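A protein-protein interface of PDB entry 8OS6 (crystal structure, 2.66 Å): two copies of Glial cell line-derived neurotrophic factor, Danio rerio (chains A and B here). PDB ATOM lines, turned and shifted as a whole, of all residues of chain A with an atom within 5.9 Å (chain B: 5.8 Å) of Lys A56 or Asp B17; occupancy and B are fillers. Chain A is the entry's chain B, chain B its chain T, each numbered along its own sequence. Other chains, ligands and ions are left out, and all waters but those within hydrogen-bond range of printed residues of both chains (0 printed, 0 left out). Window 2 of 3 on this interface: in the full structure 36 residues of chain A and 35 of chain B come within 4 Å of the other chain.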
ATOM      1  N   ASN A  50      33.652  28.788  -7.673  1.00  0.00           N
ATOM      2  CA  ASN A  50      32.228  28.581  -7.917  1.00  0.00           C
ATOM      3  C   ASN A  50      31.377  29.154  -6.789  1.00  0.00           C
ATOM      4  O   ASN A  50      30.305  29.717  -7.041  1.00  0.00           O
ATOM      5  CB  ASN A  50      31.938  27.091  -8.101  1.00  0.00           C
ATOM      6  CG  ASN A  50      32.574  26.525  -9.357  1.00  0.00           C
ATOM      7  OD1 ASN A  50      33.567  27.053  -9.857  1.00  0.00           O
ATOM      8  ND2 ASN A  50      31.998  25.446  -9.876  1.00  0.00           N
ATOM      9  N   LEU A  51      31.833  29.023  -5.540  1.00  0.00           N
ATOM     10  CA  LEU A  51      31.079  29.578  -4.420  1.00  0.00           C
ATOM     11  C   LEU A  51      31.005  31.098  -4.501  1.00  0.00           C
ATOM     12  O   LEU A  51      29.946  31.688  -4.256  1.00  0.00           O
ATOM     13  CB  LEU A  51      31.710  29.147  -3.096  1.00  0.00           C
ATOM     14  CG  LEU A  51      31.302  27.778  -2.549  1.00  0.00           C
ATOM     15  CD1 LEU A  51      32.090  27.444  -1.289  1.00  0.00           C
ATOM     16  CD2 LEU A  51      29.805  27.736  -2.273  1.00  0.00           C
ATOM     17  N   THR A  52      32.122  31.752  -4.837  1.00  0.00           N
ATOM     18  CA  THR A  52      32.135  33.209  -4.933  1.00  0.00           C
ATOM     19  C   THR A  52      31.138  33.700  -5.977  1.00  0.00           C
ATOM     20  O   THR A  52      30.376  34.642  -5.733  1.00  0.00           O
ATOM     21  CB  THR A  52      33.544  33.708  -5.270  1.00  0.00           C
ATOM     22  OG1 THR A  52      34.053  32.995  -6.405  1.00  0.00           O
ATOM     23  CG2 THR A  52      34.487  33.518  -4.089  1.00  0.00           C
ATOM     24  N   HIS A  53      31.140  33.075  -7.157  1.00  0.00           N
ATOM     25  CA  HIS A  53      30.172  33.433  -8.190  1.00  0.00           C
ATOM     26  C   HIS A  53      28.745  33.180  -7.713  1.00  0.00           C
ATOM     27  O   HIS A  53      27.824  33.930  -8.058  1.00  0.00           O
ATOM     28  CB  HIS A  53      30.464  32.643  -9.467  1.00  0.00           C
ATOM     29  CG  HIS A  53      29.824  33.214 -10.695  1.00  0.00           C
ATOM     30  ND1 HIS A  53      30.552  33.602 -11.800  1.00  0.00           N
ATOM     31  CD2 HIS A  53      28.526  33.453 -10.997  1.00  0.00           C
ATOM     32  CE1 HIS A  53      29.731  34.061 -12.727  1.00  0.00           C
ATOM     33  NE2 HIS A  53      28.496  33.982 -12.265  1.00  0.00           N
ATOM     34  N   ASN A  54      28.544  32.127  -6.916  1.00  0.00           N
ATOM     35  CA  ASN A  54      27.230  31.868  -6.338  1.00  0.00           C
ATOM     36  C   ASN A  54      26.878  32.859  -5.236  1.00  0.00           C
ATOM     37  O   ASN A  54      25.695  33.015  -4.913  1.00  0.00           O
ATOM     38  CB  ASN A  54      27.167  30.444  -5.778  1.00  0.00           C
ATOM     39  CG  ASN A  54      27.197  29.388  -6.864  1.00  0.00           C
ATOM     40  OD1 ASN A  54      27.673  29.633  -7.973  1.00  0.00           O
ATOM     41  ND2 ASN A  54      26.687  28.202  -6.549  1.00  0.00           N
ATOM     42  N   LYS A  55      27.873  33.525  -4.651  1.00  0.00           N
ATOM     43  CA  LYS A  55      27.719  34.513  -3.586  1.00  0.00           C
ATOM     44  C   LYS A  55      27.470  33.863  -2.232  1.00  0.00           C
ATOM     45  O   LYS A  55      27.221  34.581  -1.249  1.00  0.00           O
ATOM     46  CB  LYS A  55      26.585  35.501  -3.880  1.00  0.00           C
ATOM     47  N   LYS A  56      27.531  32.532  -2.139  1.00  0.00           N
ATOM     48  CA  LYS A  56      27.358  31.876  -0.847  1.00  0.00           C
ATOM     49  C   LYS A  56      28.404  32.350   0.154  1.00  0.00           C
ATOM     50  O   LYS A  56      28.084  32.617   1.318  1.00  0.00           O
ATOM     51  CB  LYS A  56      27.415  30.358  -1.021  1.00  0.00           C
ATOM     52  CG  LYS A  56      26.058  29.709  -1.283  1.00  0.00           C
ATOM     53  CD  LYS A  56      25.402  29.262   0.018  1.00  0.00           C
ATOM     54  CE  LYS A  56      23.906  29.020  -0.149  1.00  0.00           C
ATOM     55  NZ  LYS A  56      23.589  27.711  -0.787  1.00  0.00           N
ATOM     56  N   LEU A  57      29.657  32.468  -0.278  1.00  0.00           N
ATOM     57  CA  LEU A  57      30.725  33.034   0.546  1.00  0.00           C
ATOM     58  C   LEU A  57      30.941  34.467   0.067  1.00  0.00           C
ATOM     59  O   LEU A  57      31.634  34.703  -0.925  1.00  0.00           O
ATOM     60  CB  LEU A  57      31.995  32.199   0.442  1.00  0.00           C
ATOM     61  CG  LEU A  57      32.976  32.301   1.613  1.00  0.00           C
ATOM     62  CD1 LEU A  57      32.347  31.801   2.908  1.00  0.00           C
ATOM     63  CD2 LEU A  57      34.247  31.522   1.296  1.00  0.00           C
ATOM     64  N   ASP A  58      30.334  35.423   0.772  1.00  0.00           N
ATOM     65  CA  ASP A  58      30.327  36.822   0.364  1.00  0.00           C
ATOM     66  C   ASP A  58      31.198  37.705   1.244  1.00  0.00           C
ATOM     67  O   ASP A  58      31.983  38.508   0.731  1.00  0.00           O
ATOM     68  CB  ASP A  58      28.886  37.355   0.364  1.00  0.00           C
ATOM     69  N   ILE B  11      31.868  26.148   6.888  1.00  0.00           N
ATOM     70  CA  ILE B  11      30.609  26.485   6.232  1.00  0.00           C
ATOM     71  C   ILE B  11      29.878  25.186   5.919  1.00  0.00           C
ATOM     72  O   ILE B  11      30.501  24.161   5.628  1.00  0.00           O
ATOM     73  CB  ILE B  11      30.858  27.346   4.967  1.00  0.00           C
ATOM     74  CG1 ILE B  11      29.539  27.714   4.284  1.00  0.00           C
ATOM     75  CG2 ILE B  11      31.774  26.625   3.994  1.00  0.00           C
ATOM     76  CD1 ILE B  11      28.625  28.569   5.131  1.00  0.00           C
ATOM     77  N   HIS B  12      28.546  25.230   5.992  1.00  0.00           N
ATOM     78  CA  HIS B  12      27.684  24.059   5.839  1.00  0.00           C
ATOM     79  C   HIS B  12      26.840  24.238   4.584  1.00  0.00           C
ATOM     80  O   HIS B  12      26.059  25.192   4.491  1.00  0.00           O
ATOM     81  CB  HIS B  12      26.798  23.882   7.075  1.00  0.00           C
ATOM     82  CG  HIS B  12      25.934  22.658   7.045  1.00  0.00           C
ATOM     83  ND1 HIS B  12      25.025  22.408   6.039  1.00  0.00           N
ATOM     84  CD2 HIS B  12      25.821  21.627   7.916  1.00  0.00           C
ATOM     85  CE1 HIS B  12      24.403  21.268   6.282  1.00  0.00           C
ATOM     86  NE2 HIS B  12      24.867  20.774   7.416  1.00  0.00           N
ATOM     87  N   LEU B  13      26.986  23.318   3.631  1.00  0.00           N
ATOM     88  CA  LEU B  13      26.409  23.480   2.303  1.00  0.00           C
ATOM     89  C   LEU B  13      25.898  22.140   1.795  1.00  0.00           C
ATOM     90  O   LEU B  13      26.254  21.081   2.318  1.00  0.00           O
ATOM     91  CB  LEU B  13      27.444  24.040   1.318  1.00  0.00           C
ATOM     92  CG  LEU B  13      28.239  25.253   1.801  1.00  0.00           C
ATOM     93  CD1 LEU B  13      29.498  25.440   0.974  1.00  0.00           C
ATOM     94  CD2 LEU B  13      27.368  26.498   1.745  1.00  0.00           C
ATOM     95  N   ASN B  14      25.054  22.194   0.765  1.00  0.00           N
ATOM     96  CA  ASN B  14      24.726  20.971   0.059  1.00  0.00           C
ATOM     97  C   ASN B  14      25.820  20.649  -0.961  1.00  0.00           C
ATOM     98  O   ASN B  14      26.599  21.516  -1.367  1.00  0.00           O
ATOM     99  CB  ASN B  14      23.402  21.057  -0.692  1.00  0.00           C
ATOM    100  CG  ASN B  14      22.410  22.060  -0.119  1.00  0.00           C
ATOM    101  OD1 ASN B  14      22.299  23.179  -0.619  1.00  0.00           O
ATOM    102  ND2 ASN B  14      21.658  21.655   0.900  1.00  0.00           N
ATOM    103  N   VAL B  15      25.859  19.388  -1.397  1.00  0.00           N
ATOM    104  CA  VAL B  15      26.805  19.010  -2.444  1.00  0.00           C
ATOM    105  C   VAL B  15      26.508  19.770  -3.730  1.00  0.00           C
ATOM    106  O   VAL B  15      27.419  20.060  -4.514  1.00  0.00           O
ATOM    107  CB  VAL B  15      26.776  17.487  -2.681  1.00  0.00           C
ATOM    108  CG1 VAL B  15      27.723  17.106  -3.816  1.00  0.00           C
ATOM    109  CG2 VAL B  15      27.133  16.741  -1.405  1.00  0.00           C
ATOM    110  N   THR B  16      25.239  20.104  -3.970  1.00  0.00           N
ATOM    111  CA  THR B  16      24.876  20.807  -5.193  1.00  0.00           C
ATOM    112  C   THR B  16      25.246  22.284  -5.148  1.00  0.00           C
ATOM    113  O   THR B  16      25.363  22.910  -6.208  1.00  0.00           O
ATOM    114  CB  THR B  16      23.376  20.655  -5.466  1.00  0.00           C
ATOM    115  OG1 THR B  16      23.094  21.030  -6.821  1.00  0.00           O
ATOM    116  CG2 THR B  16      22.558  21.530  -4.523  1.00  0.00           C
ATOM    117  N   ASP B  17      25.432  22.853  -3.953  1.00  0.00           N
ATOM    118  CA  ASP B  17      25.834  24.253  -3.855  1.00  0.00           C
ATOM    119  C   ASP B  17      27.239  24.472  -4.399  1.00  0.00           C
ATOM    120  O   ASP B  17      27.527  25.536  -4.961  1.00  0.00           O
ATOM    121  CB  ASP B  17      25.761  24.725  -2.402  1.00  0.00           C
ATOM    122  CG  ASP B  17      24.337  24.840  -1.891  1.00  0.00           C
ATOM    123  OD1 ASP B  17      23.394  24.637  -2.686  1.00  0.00           O
ATOM    124  OD2 ASP B  17      24.163  25.135  -0.688  1.00  0.00           O
ATOM    125  N   LEU B  18      28.128  23.490  -4.236  1.00  0.00           N
ATOM    126  CA  LEU B  18      29.480  23.621  -4.762  1.00  0.00           C
ATOM    127  C   LEU B  18      29.487  23.827  -6.270  1.00  0.00           C
ATOM    128  O   LEU B  18      30.455  24.377  -6.807  1.00  0.00           O
ATOM    129  CB  LEU B  18      30.306  22.386  -4.402  1.00  0.00           C
ATOM    130  CG  LEU B  18      30.294  21.971  -2.928  1.00  0.00           C
ATOM    131  CD1 LEU B  18      31.435  21.003  -2.637  1.00  0.00           C
ATOM    132  CD2 LEU B  18      30.361  23.183  -2.009  1.00  0.00           C
ATOM    133  N   ASP B  19      28.435  23.396  -6.966  1.00  0.00           N
ATOM    134  CA  ASP B  19      28.298  23.630  -8.403  1.00  0.00           C
ATOM    135  C   ASP B  19      29.449  22.987  -9.174  1.00  0.00           C
ATOM    136  O   ASP B  19      30.127  23.628  -9.980  1.00  0.00           O
ATOM    137  CB  ASP B  19      28.206  25.129  -8.698  1.00  0.00           C
ATOM    138  CG  ASP B  19      27.876  25.421 -10.147  1.00  0.00           C
ATOM    139  OD1 ASP B  19      26.791  25.004 -10.604  1.00  0.00           O
ATOM    140  OD2 ASP B  19      28.698  26.072 -10.827  1.00  0.00           O
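OD2 of Asp B17 is in salt-bridge range of NZ of Lys A56 (2.6 Å). ND2 of Asn A50 lies within hydrogen-bond range of O of Asp B19 (2.6 Å). The side-chain amide nitrogen of Asn A54 lies within hydrogen-bond range of the backbone carbonyl oxygen of Asp B17 (3.2 Å).
The backbone carbonyl oxygen (O) of Leu A51 lies within hydrogen-bond range of the backbone NH (N) of Lys A56 (3.3 Å). The side-chain carboxylate (OD2) of Asp B17 lies close to the side-chain amide oxygen (OD1) of Asn B14 (2.7 Å). O of Asn A50 lies close to OD1 of Asn A54.
Among the printed residues, pairs that only touch across the chains: Asn A50 with Leu B18 (3.4 Å), Leu A51 with Leu B13 (3.98 Å) and Lys A56 with Leu B13 (3.8 Å).
Of the printed residues of chain B, Asn A50 touches Leu B18 and Asp B19. Printed residues of chain B within 4 Å of Asn A54: Asp B17. Lys A56 touches two residues of chain B. Thr B16 touches none of the printed residues of chain A. Printed residues of chain A within 4 Å of Leu B18: Asn A50 (3.4 Å). Printed residues of chain A within 4 Å of Asp B19: Asn A50. The nearest residue of chain B that does not touch Lys A56 is Asn B14 (4.7 Å). The nearest printed residue of chain B that does not touch Asn A50 is Asp B17 (5.4 Å).
Printed residues of chain B that touch a printed residue of chain A: Leu B13, Asp B17, Leu B18 and Asp B19. Hydrophobic or aromatic side chains of chain B that line the printed part of chain A: Leu B13. Printed residues of chain A that touch a printed residue of chain B: Asn A50, Leu A51, Asn A54 and Lys A56. Hydrophobic or aromatic side chains of chain A that line the printed part of chain B: Leu A51. Among the printed residues, 6 pairs touch across the chains. Among the printed residues, Asp or Glu carboxylates within 4 Å of a Lys or Arg side-chain nitrogen of the other chain: Lys A56 with Asp B17 (2.6 Å).
No position is printed for both chains. Of the 6 pairs that touch across the chains among the printed residues, none has its exchanged pair printed and touching as well.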
